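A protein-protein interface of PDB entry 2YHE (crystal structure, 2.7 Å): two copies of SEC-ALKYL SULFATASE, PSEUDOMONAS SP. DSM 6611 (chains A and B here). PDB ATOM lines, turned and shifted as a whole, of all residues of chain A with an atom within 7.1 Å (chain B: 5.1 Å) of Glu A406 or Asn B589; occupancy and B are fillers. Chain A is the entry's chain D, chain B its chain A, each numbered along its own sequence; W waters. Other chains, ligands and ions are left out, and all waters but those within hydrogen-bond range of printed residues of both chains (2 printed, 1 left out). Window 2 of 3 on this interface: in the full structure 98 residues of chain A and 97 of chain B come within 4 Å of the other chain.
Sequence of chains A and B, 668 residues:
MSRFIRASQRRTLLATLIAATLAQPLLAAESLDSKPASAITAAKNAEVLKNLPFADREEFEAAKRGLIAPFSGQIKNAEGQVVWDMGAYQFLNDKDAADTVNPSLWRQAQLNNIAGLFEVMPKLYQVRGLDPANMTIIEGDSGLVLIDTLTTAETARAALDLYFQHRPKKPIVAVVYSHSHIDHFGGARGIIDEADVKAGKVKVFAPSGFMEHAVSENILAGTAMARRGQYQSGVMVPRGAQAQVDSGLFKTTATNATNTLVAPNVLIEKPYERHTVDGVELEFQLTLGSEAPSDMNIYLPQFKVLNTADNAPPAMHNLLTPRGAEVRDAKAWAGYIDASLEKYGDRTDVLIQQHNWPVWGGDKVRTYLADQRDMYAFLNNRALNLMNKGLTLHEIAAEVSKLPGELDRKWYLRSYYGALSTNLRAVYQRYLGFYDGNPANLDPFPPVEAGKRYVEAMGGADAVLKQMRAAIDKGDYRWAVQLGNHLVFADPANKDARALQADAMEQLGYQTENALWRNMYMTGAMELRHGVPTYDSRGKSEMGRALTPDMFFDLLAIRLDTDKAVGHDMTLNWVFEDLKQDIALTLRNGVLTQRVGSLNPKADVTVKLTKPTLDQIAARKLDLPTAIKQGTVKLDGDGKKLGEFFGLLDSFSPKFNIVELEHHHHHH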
ATOM      1  N   ALA A 370       8.891  -8.577 -23.420  1.00  0.00           N
ATOM      2  CA  ALA A 370       9.924  -8.303 -22.423  1.00  0.00           C
ATOM      3  C   ALA A 370       9.289  -7.668 -21.165  1.00  0.00           C
ATOM      4  O   ALA A 370       9.607  -8.062 -20.049  1.00  0.00           O
ATOM      5  CB  ALA A 370      10.979  -7.388 -23.013  1.00  0.00           C
ATOM      6  N   ASP A 371       8.345  -6.738 -21.370  1.00  0.00           N
ATOM      7  CA  ASP A 371       7.610  -6.049 -20.310  1.00  0.00           C
ATOM      8  C   ASP A 371       6.749  -7.044 -19.522  1.00  0.00           C
ATOM      9  O   ASP A 371       6.797  -7.057 -18.287  1.00  0.00           O
ATOM     10  CB  ASP A 371       6.768  -4.899 -20.890  1.00  0.00           C
ATOM     11  CG  ASP A 371       7.554  -3.650 -21.265  1.00  0.00           C
ATOM     12  OD1 ASP A 371       8.695  -3.494 -20.780  1.00  0.00           O
ATOM     13  OD2 ASP A 371       6.998  -2.792 -21.981  1.00  0.00           O
ATOM     14  N   ASP A 374       8.945  -9.434 -17.401  1.00  0.00           N
ATOM     15  CA  ASP A 374       9.445  -8.709 -16.237  1.00  0.00           C
ATOM     16  C   ASP A 374       8.405  -8.543 -15.151  1.00  0.00           C
ATOM     17  O   ASP A 374       8.730  -8.759 -13.983  1.00  0.00           O
ATOM     18  CB  ASP A 374      10.070  -7.379 -16.660  1.00  0.00           C
ATOM     19  CG  ASP A 374      11.386  -7.513 -17.442  1.00  0.00           C
ATOM     20  OD1 ASP A 374      11.940  -8.638 -17.510  1.00  0.00           O
ATOM     21  OD2 ASP A 374      11.870  -6.496 -17.949  1.00  0.00           O
ATOM     22  N   PHE A 378       8.925 -10.160 -11.579  1.00  0.00           N
ATOM     23  CA  PHE A 378       8.915  -9.244 -10.445  1.00  0.00           C
ATOM     24  C   PHE A 378       7.942  -9.738  -9.373  1.00  0.00           C
ATOM     25  O   PHE A 378       8.315  -9.826  -8.194  1.00  0.00           O
ATOM     26  CB  PHE A 378       8.553  -7.832 -10.900  1.00  0.00           C
ATOM     27  CG  PHE A 378       8.205  -6.887  -9.776  1.00  0.00           C
ATOM     28  CD1 PHE A 378       9.205  -6.326  -8.978  1.00  0.00           C
ATOM     29  CD2 PHE A 378       6.870  -6.582  -9.484  1.00  0.00           C
ATOM     30  CE1 PHE A 378       8.880  -5.448  -7.940  1.00  0.00           C
ATOM     31  CE2 PHE A 378       6.545  -5.717  -8.431  1.00  0.00           C
ATOM     32  CZ  PHE A 378       7.553  -5.155  -7.675  1.00  0.00           C
ATOM     33  N   LYS A 402       3.483  -0.460  -6.474  1.00  0.00           N
ATOM     34  CA  LYS A 402       3.523  -0.363  -7.940  1.00  0.00           C
ATOM     35  C   LYS A 402       4.564  -1.269  -8.598  1.00  0.00           C
ATOM     36  O   LYS A 402       5.464  -1.783  -7.929  1.00  0.00           O
ATOM     37  CB  LYS A 402       3.738   1.107  -8.391  1.00  0.00           C
ATOM     38  CG  LYS A 402       4.868   1.852  -7.672  1.00  0.00           C
ATOM     39  CD  LYS A 402       5.232   3.176  -8.350  1.00  0.00           C
ATOM     40  CE  LYS A 402       6.712   3.254  -8.671  1.00  0.00           C
ATOM     41  NZ  LYS A 402       7.097   2.513  -9.910  1.00  0.00           N
ATOM     42  N   LEU A 403       4.450  -1.428  -9.930  1.00  0.00           N
ATOM     43  CA  LEU A 403       5.426  -2.161 -10.737  1.00  0.00           C
ATOM     44  C   LEU A 403       6.721  -1.315 -10.817  1.00  0.00           C
ATOM     45  O   LEU A 403       6.657  -0.088 -10.723  1.00  0.00           O
ATOM     46  CB  LEU A 403       4.880  -2.483 -12.149  1.00  0.00           C
ATOM     47  CG  LEU A 403       3.782  -3.550 -12.243  1.00  0.00           C
ATOM     48  CD1 LEU A 403       3.410  -3.810 -13.666  1.00  0.00           C
ATOM     49  CD2 LEU A 403       4.170  -4.855 -11.549  1.00  0.00           C
ATOM     50  N   PRO A 404       7.902  -1.939 -10.897  1.00  0.00           N
ATOM     51  CA  PRO A 404       9.140  -1.147 -10.872  1.00  0.00           C
ATOM     52  C   PRO A 404       9.550  -0.503 -12.199  1.00  0.00           C
ATOM     53  O   PRO A 404       9.192  -1.001 -13.286  1.00  0.00           O
ATOM     54  CB  PRO A 404      10.178  -2.159 -10.390  1.00  0.00           C
ATOM     55  CG  PRO A 404       9.708  -3.458 -10.940  1.00  0.00           C
ATOM     56  CD  PRO A 404       8.190  -3.389 -10.972  1.00  0.00           C
ATOM     57  N   GLY A 405      10.319   0.587 -12.086  1.00  0.00           N
ATOM     58  CA  GLY A 405      10.837   1.344 -13.220  1.00  0.00           C
ATOM     59  C   GLY A 405       9.800   1.695 -14.268  1.00  0.00           C
ATOM     60  O   GLY A 405       8.729   2.210 -13.930  1.00  0.00           O
ATOM     61  N   GLU A 406      10.103   1.372 -15.540  1.00  0.00           N
ATOM     62  CA  GLU A 406       9.254   1.678 -16.692  1.00  0.00           C
ATOM     63  C   GLU A 406       7.975   0.874 -16.783  1.00  0.00           C
ATOM     64  O   GLU A 406       7.083   1.244 -17.565  1.00  0.00           O
ATOM     65  CB  GLU A 406      10.042   1.569 -18.001  1.00  0.00           C
ATOM     66  CG  GLU A 406      10.997   2.733 -18.232  1.00  0.00           C
ATOM     67  CD  GLU A 406      10.430   4.111 -17.936  1.00  0.00           C
ATOM     68  OE1 GLU A 406       9.444   4.526 -18.596  1.00  0.00           O
ATOM     69  OE2 GLU A 406      10.951   4.759 -17.000  1.00  0.00           O
ATOM     70  N   LEU A 407       7.871  -0.227 -15.984  1.00  0.00           N
ATOM     71  CA  LEU A 407       6.693  -1.098 -15.998  1.00  0.00           C
ATOM     72  C   LEU A 407       5.466  -0.380 -15.492  1.00  0.00           C
ATOM     73  O   LEU A 407       4.361  -0.661 -15.961  1.00  0.00           O
ATOM     74  CB  LEU A 407       6.928  -2.416 -15.255  1.00  0.00           C
ATOM     75  CG  LEU A 407       8.138  -3.252 -15.684  1.00  0.00           C
ATOM     76  CD1 LEU A 407       8.342  -4.422 -14.742  1.00  0.00           C
ATOM     77  CD2 LEU A 407       8.061  -3.692 -17.144  1.00  0.00           C
ATOM     78  N   ASP A 408       5.665   0.599 -14.597  1.00  0.00           N
ATOM     79  CA  ASP A 408       4.580   1.414 -14.069  1.00  0.00           C
ATOM     80  C   ASP A 408       4.033   2.389 -15.140  1.00  0.00           C
ATOM     81  O   ASP A 408       2.902   2.872 -15.009  1.00  0.00           O
ATOM     82  CB  ASP A 408       5.058   2.182 -12.828  1.00  0.00           C
ATOM     83  CG  ASP A 408       3.981   3.013 -12.142  1.00  0.00           C
ATOM     84  OD1 ASP A 408       2.933   2.437 -11.761  1.00  0.00           O
ATOM     85  OD2 ASP A 408       4.192   4.241 -11.975  1.00  0.00           O
ATOM     86  N   ARG A 409       4.815   2.643 -16.207  1.00  0.00           N
ATOM     87  CA  ARG A 409       4.431   3.582 -17.263  1.00  0.00           C
ATOM     88  C   ARG A 409       3.659   3.008 -18.476  1.00  0.00           C
ATOM     89  O   ARG A 409       3.114   3.788 -19.281  1.00  0.00           O
ATOM     90  CB  ARG A 409       5.630   4.444 -17.678  1.00  0.00           C
ATOM     91  CG  ARG A 409       5.795   5.697 -16.837  1.00  0.00           C
ATOM     92  CD  ARG A 409       7.216   5.861 -16.352  1.00  0.00           C
ATOM     93  NE  ARG A 409       7.347   5.552 -14.926  1.00  0.00           N
ATOM     94  CZ  ARG A 409       8.492   5.594 -14.246  1.00  0.00           C
ATOM     95  NH1 ARG A 409       9.623   5.940 -14.854  1.00  0.00           N
ATOM     96  NH2 ARG A 409       8.518   5.287 -12.956  1.00  0.00           N
ATOM     97  N   LYS A 410       3.543   1.665 -18.568  1.00  0.00           N
ATOM     98  CA  LYS A 410       2.853   0.995 -19.678  1.00  0.00           C
ATOM     99  C   LYS A 410       1.363   0.774 -19.408  1.00  0.00           C
ATOM    100  O   LYS A 410       1.009   0.295 -18.333  1.00  0.00           O
ATOM    101  CB  LYS A 410       3.559  -0.325 -20.030  1.00  0.00           C
ATOM    102  CG  LYS A 410       5.092  -0.270 -19.971  1.00  0.00           C
ATOM    103  CD  LYS A 410       5.706   0.476 -21.133  1.00  0.00           C
ATOM    104  CE  LYS A 410       7.192   0.670 -20.958  1.00  0.00           C
ATOM    105  NZ  LYS A 410       7.948   0.291 -22.182  1.00  0.00           N
ATOM    106  N   LEU A 413       0.117  -3.005 -18.823  1.00  0.00           N
ATOM    107  CA  LEU A 413       0.592  -3.647 -17.601  1.00  0.00           C
ATOM    108  C   LEU A 413      -0.203  -3.197 -16.366  1.00  0.00           C
ATOM    109  O   LEU A 413       0.118  -3.625 -15.249  1.00  0.00           O
ATOM    110  CB  LEU A 413       2.113  -3.452 -17.402  1.00  0.00           C
ATOM    111  CG  LEU A 413       3.075  -3.951 -18.496  1.00  0.00           C
ATOM    112  CD1 LEU A 413       4.474  -3.537 -18.190  1.00  0.00           C
ATOM    113  CD2 LEU A 413       3.056  -5.448 -18.632  1.00  0.00           C
ATOM    114  N   THR B 562      15.292  -4.787  -5.896  1.00  0.00           N
ATOM    115  CA  THR B 562      14.632  -4.079  -7.007  1.00  0.00           C
ATOM    116  C   THR B 562      14.719  -2.541  -6.874  1.00  0.00           C
ATOM    117  O   THR B 562      15.009  -1.863  -7.854  1.00  0.00           O
ATOM    118  CB  THR B 562      13.177  -4.591  -7.179  1.00  0.00           C
ATOM    119  OG1 THR B 562      13.200  -5.980  -7.475  1.00  0.00           O
ATOM    120  CG2 THR B 562      12.412  -3.863  -8.250  1.00  0.00           C
ATOM    121  N   VAL B 566      16.755  -0.441  -9.754  1.00  0.00           N
ATOM    122  CA  VAL B 566      16.079   0.409 -10.728  1.00  0.00           C
ATOM    123  C   VAL B 566      17.016   1.567 -11.100  1.00  0.00           C
ATOM    124  O   VAL B 566      17.568   2.224 -10.213  1.00  0.00           O
ATOM    125  CB  VAL B 566      14.644   0.856 -10.296  1.00  0.00           C
ATOM    126  CG1 VAL B 566      14.124   2.036 -11.132  1.00  0.00           C
ATOM    127  CG2 VAL B 566      13.664  -0.326 -10.364  1.00  0.00           C
ATOM    128  N   ASP B 569      19.911  -0.790 -15.350  1.00  0.00           N
ATOM    129  CA  ASP B 569      19.743  -1.806 -16.387  1.00  0.00           C
ATOM    130  C   ASP B 569      21.108  -2.201 -16.958  1.00  0.00           C
ATOM    131  O   ASP B 569      21.954  -1.336 -17.237  1.00  0.00           O
ATOM    132  CB  ASP B 569      18.831  -1.317 -17.517  1.00  0.00           C
ATOM    133  CG  ASP B 569      17.362  -1.184 -17.174  1.00  0.00           C
ATOM    134  OD1 ASP B 569      17.034  -1.108 -15.957  1.00  0.00           O
ATOM    135  OD2 ASP B 569      16.536  -1.129 -18.124  1.00  0.00           O
ATOM    136  N   LEU B 587      19.248  -7.629 -16.445  1.00  0.00           N
ATOM    137  CA  LEU B 587      18.685  -6.820 -15.375  1.00  0.00           C
ATOM    138  C   LEU B 587      17.961  -5.628 -16.027  1.00  0.00           C
ATOM    139  O   LEU B 587      18.599  -4.785 -16.662  1.00  0.00           O
ATOM    140  CB  LEU B 587      19.772  -6.347 -14.405  1.00  0.00           C
ATOM    141  CG  LEU B 587      19.324  -5.390 -13.294  1.00  0.00           C
ATOM    142  CD1 LEU B 587      18.290  -6.043 -12.373  1.00  0.00           C
ATOM    143  CD2 LEU B 587      20.521  -4.908 -12.503  1.00  0.00           C
ATOM    144  N   ARG B 588      16.626  -5.599 -15.915  1.00  0.00           N
ATOM    145  CA  ARG B 588      15.782  -4.561 -16.509  1.00  0.00           C
ATOM    146  C   ARG B 588      14.699  -4.167 -15.529  1.00  0.00           C
ATOM    147  O   ARG B 588      13.983  -5.035 -15.037  1.00  0.00           O
ATOM    148  CB  ARG B 588      15.160  -5.091 -17.817  1.00  0.00           C
ATOM    149  CG  ARG B 588      14.870  -4.026 -18.846  1.00  0.00           C
ATOM    150  CD  ARG B 588      14.434  -4.643 -20.158  1.00  0.00           C
ATOM    151  NE  ARG B 588      13.014  -4.939 -20.135  1.00  0.00           N
ATOM    152  CZ  ARG B 588      12.114  -4.399 -20.946  1.00  0.00           C
ATOM    153  NH1 ARG B 588      12.493  -3.558 -21.906  1.00  0.00           N
ATOM    154  NH2 ARG B 588      10.834  -4.729 -20.835  1.00  0.00           N
ATOM    155  N   ASN B 589      14.586  -2.865 -15.235  1.00  0.00           N
ATOM    156  CA  ASN B 589      13.605  -2.278 -14.295  1.00  0.00           C
ATOM    157  C   ASN B 589      13.673  -2.934 -12.919  1.00  0.00           C
ATOM    158  O   ASN B 589      12.642  -3.158 -12.283  1.00  0.00           O
ATOM    159  CB  ASN B 589      12.173  -2.342 -14.841  1.00  0.00           C
ATOM    160  CG  ASN B 589      11.991  -1.629 -16.156  1.00  0.00           C
ATOM    161  OD1 ASN B 589      12.203  -0.400 -16.252  1.00  0.00           O
ATOM    162  ND2 ASN B 589      11.572  -2.383 -17.184  1.00  0.00           N
ATOM    163  N   GLY B 590      14.886  -3.269 -12.491  1.00  0.00           N
ATOM    164  CA  GLY B 590      15.120  -3.921 -11.215  1.00  0.00           C
ATOM    165  C   GLY B 590      14.648  -5.365 -11.179  1.00  0.00           C
ATOM    166  O   GLY B 590      14.373  -5.886 -10.093  1.00  0.00           O
ATOM    167  N   VAL B 591      14.510  -6.001 -12.361  1.00  0.00           N
ATOM    168  CA  VAL B 591      14.047  -7.378 -12.507  1.00  0.00           C
ATOM    169  C   VAL B 591      15.160  -8.215 -13.166  1.00  0.00           C
ATOM    170  O   VAL B 591      15.636  -7.880 -14.257  1.00  0.00           O
ATOM    171  CB  VAL B 591      12.677  -7.524 -13.240  1.00  0.00           C
ATOM    172  CG1 VAL B 591      12.189  -8.958 -13.185  1.00  0.00           C
ATOM    173  CG2 VAL B 591      11.612  -6.593 -12.671  1.00  0.00           C
HETATM  174  O   HOH W   1      14.432  -9.066 -16.771  1.00  0.00           O
HETATM  175  O   HOH W   2      10.778  -1.789 -19.864  1.00  0.00           O
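No position is printed for both chains.
The guanidinium group (NH2) of Arg B588 is in salt-bridge range of the side-chain carboxylate (OD1) of Asp A371, 2.5 Å away.
The guanidinium group (NE) of Arg B588 lies within salt-bridge range of the side-chain carboxylate (OD2) of Asp A374 (2.9 Å).
The backbone NH (N) of Glu A406 is in hydrogen-bond range of the side-chain amide oxygen (OD1) of Asn B589 (2.8 Å).
Printed residues of chain B within 4 Å of Asp A374: Arg B588 (2.9 Å) and Val B591 (3.6 Å).
Printed residues of chain B within 4 Å of Pro A404: Thr B562, Val B566 and Asn B589.
Glu A406 touches just one residue of chain B: Asn B589 (2.8 Å).
Arg A409 touches none of the printed residues of chain B.
Printed residues of chain A within 4 Å of Val B566: Pro A404 (3.9 Å) and Gly A405 (3.9 Å).
Asp B569 touches none of the printed residues of chain A.
Printed residues of chain A within 4 Å of Arg B588: Ala A370 (3.3 Å), Asp A371 (2.5 Å) and Asp A374 (2.9 Å).
Printed residues of chain A within 4 Å of Asn B589: Pro A404 (3.2 Å), Gly A405 (3.8 Å), Glu A406 (2.8 Å) and Leu A407 (3.7 Å).
The nearest printed residue of chain B that does not touch Glu A406 is Val B566 (6.0 Å).
The nearest residue of chain A that does not touch Asn B589 is Asp A374 (4.2 Å).
The nearest printed residue of chain A that does not touch Thr B562 is Gly A405 (6.2 Å).
Water W1 lies within hydrogen-bond range of OD1 of Asp A374 (2.6 Å) and O of Val B591 (3.0 Å).
Water W2 lies within hydrogen-bond range of the side-chain carboxylate of Asp A371, the side-chain amide nitrogen of Asn B589 and the guanidinium group of Arg B588.
Of the 8 printed residues of chain B, 5 touch a printed residue of chain A.
The backbone carbonyl oxygen (O) of Gly B590 is in hydrogen-bond range of the side-chain hydroxyl (OG1) of Thr B562, at 2.9 Å.
The side-chain carboxylate (OD1) of Asp B569 is in hydrogen-bond range of the backbone NH (N) of Asn B589 (3.1 Å).
OD2 of Asp A371 is in salt-bridge range of NZ of Lys A410 (3.2 Å).
O of Gly A405 sits at hydrogen-bond distance from NH2 of Arg A409, at 3.2 Å.
OE2 of Glu A406 is in salt-bridge range of NH1 of Arg A409.
Among the printed residues, pairs that only touch across the chains: Pro A404 with Asn B589, Ala A370 with Arg B588, Pro A404 with Thr B562, Asp A374 with Val B591, Phe A378 with Val B591, Leu A407 with Asn B589, Gly A405 with Asn B589, Gly A405 with Val B566, Phe A378 with Thr B562 and Pro A404 with Val B566.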
